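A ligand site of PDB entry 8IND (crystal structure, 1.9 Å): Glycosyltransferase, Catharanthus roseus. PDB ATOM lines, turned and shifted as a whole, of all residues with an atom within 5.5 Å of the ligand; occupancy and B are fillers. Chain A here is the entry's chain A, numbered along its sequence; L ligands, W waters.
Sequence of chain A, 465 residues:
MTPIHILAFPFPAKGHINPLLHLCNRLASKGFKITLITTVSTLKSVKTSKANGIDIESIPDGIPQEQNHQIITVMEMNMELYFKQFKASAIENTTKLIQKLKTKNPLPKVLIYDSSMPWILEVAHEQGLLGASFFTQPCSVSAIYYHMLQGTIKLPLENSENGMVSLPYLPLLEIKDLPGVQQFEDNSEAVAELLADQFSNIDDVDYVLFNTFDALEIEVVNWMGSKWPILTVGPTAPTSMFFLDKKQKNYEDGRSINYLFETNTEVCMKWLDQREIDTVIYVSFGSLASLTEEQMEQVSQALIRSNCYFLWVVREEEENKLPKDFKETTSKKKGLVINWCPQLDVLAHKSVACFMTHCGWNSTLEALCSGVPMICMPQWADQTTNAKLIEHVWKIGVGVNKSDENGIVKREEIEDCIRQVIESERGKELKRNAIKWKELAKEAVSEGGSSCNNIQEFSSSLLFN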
ATOM      1  N   PHE A  11       2.627  18.531   9.507  1.00  0.00           N
ATOM      2  CA  PHE A  11       4.061  18.324   9.692  1.00  0.00           C
ATOM      3  C   PHE A  11       4.510  19.106  10.935  1.00  0.00           C
ATOM      4  O   PHE A  11       3.984  20.196  11.197  1.00  0.00           O
ATOM      5  CB  PHE A  11       4.823  18.769   8.428  1.00  0.00           C
ATOM      6  CG  PHE A  11       6.309  18.561   8.484  1.00  0.00           C
ATOM      7  CD1 PHE A  11       7.140  19.568   8.984  1.00  0.00           C
ATOM      8  CD2 PHE A  11       6.885  17.359   8.089  1.00  0.00           C
ATOM      9  CE1 PHE A  11       8.518  19.388   9.071  1.00  0.00           C
ATOM     10  CE2 PHE A  11       8.262  17.169   8.175  1.00  0.00           C
ATOM     11  CZ  PHE A  11       9.074  18.190   8.657  1.00  0.00           C
ATOM     12  N   ALA A  13       6.087  21.472  12.396  1.00  0.00           N
ATOM     13  CA  ALA A  13       6.780  22.754  12.381  1.00  0.00           C
ATOM     14  C   ALA A  13       5.724  23.851  12.292  1.00  0.00           C
ATOM     15  O   ALA A  13       4.615  23.611  11.811  1.00  0.00           O
ATOM     16  CB  ALA A  13       7.786  22.858  11.215  1.00  0.00           C
ATOM     17  N   HIS A  16       3.627  24.723   9.289  1.00  0.00           N
ATOM     18  CA  HIS A  16       2.711  23.676   8.863  1.00  0.00           C
ATOM     19  C   HIS A  16       1.548  23.501   9.828  1.00  0.00           C
ATOM     20  O   HIS A  16       0.390  23.371   9.399  1.00  0.00           O
ATOM     21  CB  HIS A  16       3.504  22.362   8.712  1.00  0.00           C
ATOM     22  CG  HIS A  16       4.557  22.449   7.655  1.00  0.00           C
ATOM     23  ND1 HIS A  16       4.414  21.888   6.402  1.00  0.00           N
ATOM     24  CD2 HIS A  16       5.746  23.111   7.641  1.00  0.00           C
ATOM     25  CE1 HIS A  16       5.478  22.189   5.672  1.00  0.00           C
ATOM     26  NE2 HIS A  16       6.297  22.918   6.402  1.00  0.00           N
ATOM     27  N   ILE A  72      12.456  19.077  15.010  1.00  0.00           N
ATOM     28  CA  ILE A  72      12.991  19.566  13.756  1.00  0.00           C
ATOM     29  C   ILE A  72      14.510  19.658  13.806  1.00  0.00           C
ATOM     30  O   ILE A  72      15.210  19.370  12.821  1.00  0.00           O
ATOM     31  CB  ILE A  72      12.358  20.928  13.413  1.00  0.00           C
ATOM     32  CG1 ILE A  72      10.898  20.713  13.049  1.00  0.00           C
ATOM     33  CG2 ILE A  72      13.124  21.607  12.315  1.00  0.00           C
ATOM     34  CD1 ILE A  72      10.715  20.141  11.663  1.00  0.00           C
ATOM     35  N   MET A  75      15.878  16.299  13.106  1.00  0.00           N
ATOM     36  CA  MET A  75      15.852  15.969  11.670  1.00  0.00           C
ATOM     37  C   MET A  75      17.019  16.566  10.913  1.00  0.00           C
ATOM     38  O   MET A  75      17.559  15.931  10.008  1.00  0.00           O
ATOM     39  CB  MET A  75      14.581  16.450  10.964  1.00  0.00           C
ATOM     40  CG  MET A  75      13.243  16.204  11.555  1.00  0.00           C
ATOM     41  SD  MET A  75      12.184  15.815  10.113  1.00  0.00           S
ATOM     42  CE  MET A  75      10.866  14.951  10.957  1.00  0.00           C
ATOM     43  N   GLU A  76      17.385  17.817  11.221  1.00  0.00           N
ATOM     44  CA  GLU A  76      18.388  18.470  10.397  1.00  0.00           C
ATOM     45  C   GLU A  76      19.753  17.808  10.551  1.00  0.00           C
ATOM     46  O   GLU A  76      20.585  17.911   9.652  1.00  0.00           O
ATOM     47  CB  GLU A  76      18.448  19.962  10.745  1.00  0.00           C
ATOM     48  CG  GLU A  76      19.487  20.769   9.959  1.00  0.00           C
ATOM     49  CD  GLU A  76      20.838  20.839  10.637  1.00  0.00           C
ATOM     50  OE1 GLU A  76      20.866  20.715  11.882  1.00  0.00           O
ATOM     51  OE2 GLU A  76      21.860  21.030   9.934  1.00  0.00           O
ATOM     52  N   MET A  79      18.706  14.488   7.625  1.00  0.00           N
ATOM     53  CA  MET A  79      17.342  14.584   7.106  1.00  0.00           C
ATOM     54  C   MET A  79      16.932  13.279   6.420  1.00  0.00           C
ATOM     55  O   MET A  79      15.820  12.780   6.614  1.00  0.00           O
ATOM     56  CB  MET A  79      17.256  15.758   6.118  1.00  0.00           C
ATOM     57  CG  MET A  79      15.854  16.255   5.754  1.00  0.00           C
ATOM     58  SD  MET A  79      14.841  16.740   7.177  1.00  0.00           S
ATOM     59  CE  MET A  79      13.402  17.414   6.359  1.00  0.00           C
ATOM     60  N   ASP A 114      -0.739  17.074   6.210  1.00  0.00           N
ATOM     61  CA  ASP A 114       0.195  17.933   5.499  1.00  0.00           C
ATOM     62  C   ASP A 114       0.674  17.258   4.215  1.00  0.00           C
ATOM     63  O   ASP A 114       1.059  16.089   4.243  1.00  0.00           O
ATOM     64  CB  ASP A 114       1.390  18.240   6.381  1.00  0.00           C
ATOM     65  CG  ASP A 114       2.213  19.386   5.840  1.00  0.00           C
ATOM     66  OD1 ASP A 114       3.004  19.197   4.878  1.00  0.00           O
ATOM     67  OD2 ASP A 114       2.049  20.498   6.373  1.00  0.00           O
ATOM     68  N   SER A 115       0.684  18.011   3.101  1.00  0.00           N
ATOM     69  CA  SER A 115       1.040  17.419   1.815  1.00  0.00           C
ATOM     70  C   SER A 115       2.456  16.842   1.798  1.00  0.00           C
ATOM     71  O   SER A 115       2.764  16.016   0.937  1.00  0.00           O
ATOM     72  CB  SER A 115       0.891  18.462   0.710  1.00  0.00           C
ATOM     73  OG  SER A 115       1.829  19.512   0.906  1.00  0.00           O
ATOM     74  N   SER A 116       3.319  17.251   2.725  1.00  0.00           N
ATOM     75  CA  SER A 116       4.667  16.700   2.811  1.00  0.00           C
ATOM     76  C   SER A 116       4.689  15.283   3.328  1.00  0.00           C
ATOM     77  O   SER A 116       5.770  14.683   3.382  1.00  0.00           O
ATOM     78  CB  SER A 116       5.549  17.554   3.718  1.00  0.00           C
ATOM     79  OG  SER A 116       5.077  17.465   5.047  1.00  0.00           O
ATOM     80  N   GLN A 137       2.041  25.572   0.638  1.00  0.00           N
ATOM     81  CA  GLN A 137       2.681  26.488  -0.284  1.00  0.00           C
ATOM     82  C   GLN A 137       1.751  26.734  -1.472  1.00  0.00           C
ATOM     83  O   GLN A 137       0.878  25.912  -1.782  1.00  0.00           O
ATOM     84  CB  GLN A 137       4.044  25.951  -0.780  1.00  0.00           C
ATOM     85  CG  GLN A 137       5.026  25.714   0.369  1.00  0.00           C
ATOM     86  CD  GLN A 137       5.499  24.247   0.447  1.00  0.00           C
ATOM     87  OE1 GLN A 137       4.702  23.303   0.336  1.00  0.00           O
ATOM     88  NE2 GLN A 137       6.825  24.059   0.652  1.00  0.00           N
ATOM     89  N   PHE A 184      21.203  23.531   2.078  1.00  0.00           N
ATOM     90  CA  PHE A 184      21.107  22.532   3.122  1.00  0.00           C
ATOM     91  C   PHE A 184      22.289  21.573   3.129  1.00  0.00           C
ATOM     92  O   PHE A 184      22.302  20.641   3.931  1.00  0.00           O
ATOM     93  CB  PHE A 184      19.788  21.780   2.983  1.00  0.00           C
ATOM     94  CG  PHE A 184      18.577  22.668   3.008  1.00  0.00           C
ATOM     95  CD1 PHE A 184      18.451  23.689   3.945  1.00  0.00           C
ATOM     96  CD2 PHE A 184      17.548  22.489   2.093  1.00  0.00           C
ATOM     97  CE1 PHE A 184      17.333  24.506   3.974  1.00  0.00           C
ATOM     98  CE2 PHE A 184      16.419  23.298   2.111  1.00  0.00           C
ATOM     99  CZ  PHE A 184      16.311  24.306   3.056  1.00  0.00           C
ATOM    100  N   ASN A 187      21.936  17.718   3.458  1.00  0.00           N
ATOM    101  CA  ASN A 187      20.499  17.458   3.462  1.00  0.00           C
ATOM    102  C   ASN A 187      19.826  17.843   2.143  1.00  0.00           C
ATOM    103  O   ASN A 187      18.610  17.665   2.019  1.00  0.00           O
ATOM    104  CB  ASN A 187      19.810  18.223   4.610  1.00  0.00           C
ATOM    105  CG  ASN A 187      20.186  17.701   5.988  1.00  0.00           C
ATOM    106  OD1 ASN A 187      20.446  16.508   6.173  1.00  0.00           O
ATOM    107  ND2 ASN A 187      20.217  18.600   6.965  1.00  0.00           N
ATOM    108  N   VAL A 191      15.958  16.806   0.977  1.00  0.00           N
ATOM    109  CA  VAL A 191      14.891  17.803   0.967  1.00  0.00           C
ATOM    110  C   VAL A 191      14.266  17.887  -0.425  1.00  0.00           C
ATOM    111  O   VAL A 191      13.039  17.974  -0.549  1.00  0.00           O
ATOM    112  CB  VAL A 191      15.418  19.160   1.440  1.00  0.00           C
ATOM    113  CG1 VAL A 191      14.359  20.226   1.176  1.00  0.00           C
ATOM    114  CG2 VAL A 191      15.793  19.102   2.930  1.00  0.00           C
ATOM    115  N   LEU A 194      11.750  15.010  -0.763  1.00  0.00           N
ATOM    116  CA  LEU A 194      10.518  15.203   0.060  1.00  0.00           C
ATOM    117  C   LEU A 194       9.585  16.194  -0.653  1.00  0.00           C
ATOM    118  O   LEU A 194       8.381  15.936  -0.705  1.00  0.00           O
ATOM    119  CB  LEU A 194      11.012  15.577   1.459  1.00  0.00           C
ATOM    120  CG  LEU A 194      10.278  16.564   2.390  1.00  0.00           C
ATOM    121  CD1 LEU A 194      10.611  18.024   2.137  1.00  0.00           C
ATOM    122  CD2 LEU A 194       8.792  16.321   2.556  1.00  0.00           C
ATOM    123  N   LEU A 195      10.148  17.259  -1.208  1.00  0.00           N
ATOM    124  CA  LEU A 195       9.319  18.277  -1.896  1.00  0.00           C
ATOM    125  C   LEU A 195       8.664  17.638  -3.127  1.00  0.00           C
ATOM    126  O   LEU A 195       7.468  17.819  -3.311  1.00  0.00           O
ATOM    127  CB  LEU A 195      10.215  19.456  -2.260  1.00  0.00           C
ATOM    128  CG  LEU A 195      10.719  20.279  -1.072  1.00  0.00           C
ATOM    129  CD1 LEU A 195      11.722  21.324  -1.520  1.00  0.00           C
ATOM    130  CD2 LEU A 195       9.576  20.915  -0.319  1.00  0.00           C
ATOM    131  N   GLN A 198       5.549  15.212  -2.672  1.00  0.00           N
ATOM    132  CA  GLN A 198       4.193  15.714  -2.410  1.00  0.00           C
ATOM    133  C   GLN A 198       3.206  15.349  -3.517  1.00  0.00           C
ATOM    134  O   GLN A 198       2.002  15.309  -3.262  1.00  0.00           O
ATOM    135  CB  GLN A 198       4.217  17.227  -2.211  1.00  0.00           C
ATOM    136  CG  GLN A 198       5.101  17.658  -1.049  1.00  0.00           C
ATOM    137  CD  GLN A 198       5.063  19.167  -0.842  1.00  0.00           C
ATOM    138  OE1 GLN A 198       4.026  19.729  -0.527  1.00  0.00           O
ATOM    139  NE2 GLN A 198       6.181  19.811  -1.081  1.00  0.00           N
ATOM    140  N   LEU A 288      12.081  28.862  11.734  1.00  0.00           N
ATOM    141  CA  LEU A 288      13.113  27.886  11.414  1.00  0.00           C
ATOM    142  C   LEU A 288      14.434  28.534  11.039  1.00  0.00           C
ATOM    143  O   LEU A 288      15.490  28.102  11.514  1.00  0.00           O
ATOM    144  CB  LEU A 288      12.624  27.018  10.251  1.00  0.00           C
ATOM    145  CG  LEU A 288      11.579  25.943  10.554  1.00  0.00           C
ATOM    146  CD1 LEU A 288      11.468  25.038   9.355  1.00  0.00           C
ATOM    147  CD2 LEU A 288      11.924  25.135  11.810  1.00  0.00           C
ATOM    148  N   ALA A 289      14.408  29.527  10.162  1.00  0.00           N
ATOM    149  CA  ALA A 289      15.633  30.119   9.658  1.00  0.00           C
ATOM    150  C   ALA A 289      16.405  30.810  10.766  1.00  0.00           C
ATOM    151  O   ALA A 289      15.839  31.394  11.696  1.00  0.00           O
ATOM    152  CB  ALA A 289      15.327  31.110   8.535  1.00  0.00           C
ATOM    153  N   TRP A 380      15.981  30.142   2.069  1.00  0.00           N
ATOM    154  CA  TRP A 380      16.114  28.834   1.423  1.00  0.00           C
ATOM    155  C   TRP A 380      14.718  28.284   1.094  1.00  0.00           C
ATOM    156  O   TRP A 380      13.700  28.922   1.356  1.00  0.00           O
ATOM    157  CB  TRP A 380      16.905  27.840   2.294  1.00  0.00           C
ATOM    158  CG  TRP A 380      16.719  27.984   3.796  1.00  0.00           C
ATOM    159  CD1 TRP A 380      17.632  28.480   4.704  1.00  0.00           C
ATOM    160  CD2 TRP A 380      15.567  27.617   4.558  1.00  0.00           C
ATOM    161  NE1 TRP A 380      17.104  28.433   5.977  1.00  0.00           N
ATOM    162  CE2 TRP A 380      15.831  27.912   5.904  1.00  0.00           C
ATOM    163  CE3 TRP A 380      14.322  27.073   4.212  1.00  0.00           C
ATOM    164  CZ2 TRP A 380      14.912  27.674   6.917  1.00  0.00           C
ATOM    165  CZ3 TRP A 380      13.403  26.825   5.223  1.00  0.00           C
ATOM    166  CH2 TRP A 380      13.698  27.127   6.561  1.00  0.00           C
ATOM    167  N   ALA A 381      14.711  27.075   0.516  1.00  0.00           N
ATOM    168  CA  ALA A 381      13.495  26.411   0.036  1.00  0.00           C
ATOM    169  C   ALA A 381      12.638  27.357  -0.791  1.00  0.00           C
ATOM    170  O   ALA A 381      13.178  28.102  -1.623  1.00  0.00           O
ATOM    171  CB  ALA A 381      12.696  25.808   1.212  1.00  0.00           C
ATOM    172  N   ASP A 382      11.319  27.356  -0.585  1.00  0.00           N
ATOM    173  CA  ASP A 382      10.422  28.117  -1.443  1.00  0.00           C
ATOM    174  C   ASP A 382      10.526  29.630  -1.222  1.00  0.00           C
ATOM    175  O   ASP A 382       9.908  30.370  -1.977  1.00  0.00           O
ATOM    176  CB  ASP A 382       8.975  27.683  -1.227  1.00  0.00           C
ATOM    177  CG  ASP A 382       8.538  27.736   0.239  1.00  0.00           C
ATOM    178  OD1 ASP A 382       9.256  27.178   1.087  1.00  0.00           O
ATOM    179  OD2 ASP A 382       7.473  28.325   0.536  1.00  0.00           O
HETATM  180  O1  LIG L   1      11.209  20.410   7.124  1.00  0.00           O
HETATM  181  C1  LIG L   1      16.024  24.613   8.560  1.00  0.00           C
HETATM  182  C2  LIG L   1      16.593  23.670   7.499  1.00  0.00           C
HETATM  183  O2  LIG L   1       8.114  21.722   2.712  1.00  0.00           O
HETATM  184  C3  LIG L   1      15.889  22.292   7.473  1.00  0.00           C
HETATM  185  O3  LIG L   1       6.892  19.988   2.213  1.00  0.00           O
HETATM  186  C4  LIG L   1      16.623  21.396   6.452  1.00  0.00           C
HETATM  187  O4  LIG L   1      17.484  23.907  10.361  1.00  0.00           O
HETATM  188  C5  LIG L   1      13.612  21.135   7.180  1.00  0.00           C
HETATM  189  C6  LIG L   1      14.392  22.468   7.082  1.00  0.00           C
HETATM  190  C7  LIG L   1      14.201  23.121   5.702  1.00  0.00           C
HETATM  191  C8  LIG L   1      12.735  23.398   5.382  1.00  0.00           C
HETATM  192  C9  LIG L   1      11.852  22.142   5.517  1.00  0.00           C
HETATM  193  C10 LIG L   1      12.074  21.146   4.354  1.00  0.00           C
HETATM  194  C11 LIG L   1      10.335  22.535   5.643  1.00  0.00           C
HETATM  195  C12 LIG L   1       9.393  21.778   4.745  1.00  0.00           C
HETATM  196  C13 LIG L   1       8.932  20.522   5.100  1.00  0.00           C
HETATM  197  C14 LIG L   1       8.059  19.843   4.252  1.00  0.00           C
HETATM  198  C15 LIG L   1       7.651  20.451   3.024  1.00  0.00           C
HETATM  199  C16 LIG L   1       8.964  22.375   3.545  1.00  0.00           C
HETATM  200  C17 LIG L   1      10.013  22.541   7.147  1.00  0.00           C
HETATM  201  C18 LIG L   1      11.072  21.686   7.786  1.00  0.00           C
HETATM  202  C19 LIG L   1      12.172  21.470   6.848  1.00  0.00           C
HETATM  203  C20 LIG L   1      16.110  24.012   9.944  1.00  0.00           C
HETATM  204  C21 LIG L   1      15.448  22.652   9.981  1.00  0.00           C
HETATM  205  C22 LIG L   1      15.954  21.688   8.897  1.00  0.00           C
HETATM  206  C23 LIG L   1      15.213  20.352   8.975  1.00  0.00           C
HETATM  207  C24 LIG L   1      13.756  20.526   8.574  1.00  0.00           C
HETATM  208  O   HOH W   1       5.251  21.914   2.336  1.00  0.00           O
HETATM  209  O   HOH W   2      17.653  23.146  13.067  1.00  0.00           O
HETATM  210  O   HOH W   3       9.571  24.254   0.858  1.00  0.00           O
HETATM  211  O   HOH W   4      18.210  26.734  11.152  1.00  0.00           O
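An oxygen (O2) of the ligand sits at hydrogen-bond distance from the side-chain amide nitrogen (NE2) of Gln 137 (3.4 Å).
The side-chain amide nitrogen of Gln 198 lies within hydrogen-bond range of an oxygen (O3) of the ligand (3.4 Å).
The side-chain hydroxyl of Ser 115 lies within hydrogen-bond range of the side-chain amide oxygen of Gln 198 (2.6 Å).
O of Glu 76 lies within hydrogen-bond range of ND2 of Asn 187 (2.8 Å).
A ring nitrogen (ND1) of His 16 sits at hydrogen-bond distance from the side-chain carboxylate (OD2) of Asp 114 (2.7 Å).
OG of Ser 116 lies within hydrogen-bond range of OD1 of Asp 114 (2.7 Å).
The backbone NH (N) of Met 79 is in hydrogen-bond range of the side-chain amide oxygen (OD1) of Asn 187 (3.0 Å).
NE2 of Gln 198 is in hydrogen-bond range of O of Leu 195 (3.3 Å).
Merely in contact with the ligand: Ser 116, Phe 11, Ile 72, Leu 195, Trp 380, Glu 76, Phe 184, Leu 288, His 16, Leu 194 and Met 79.
Within 4 Å of the ligand: Phe 11, His 16, Ile 72, Glu 76, Met 79, Ser 116, Gln 137, Phe 184, Leu 194, Leu 195, Gln 198, Leu 288 and Trp 380.
Along chain A the residues within 4 Å of the ligand span positions 11 to 380.
Water W1 bridges OE1 of Gln 137 (2.5 Å) and O3 of the ligand (2.5 Å).
Water W4 bridges O4 of the ligand (3.0 Å) and O of Leu 288 (3.1 Å).
Water W3 lies within hydrogen-bond range of the side-chain amide nitrogen of Gln 137 (2.8 Å), the side-chain carboxylate of Asp 382 (2.9 Å) and an oxygen (O2) of the ligand (3.5 Å).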
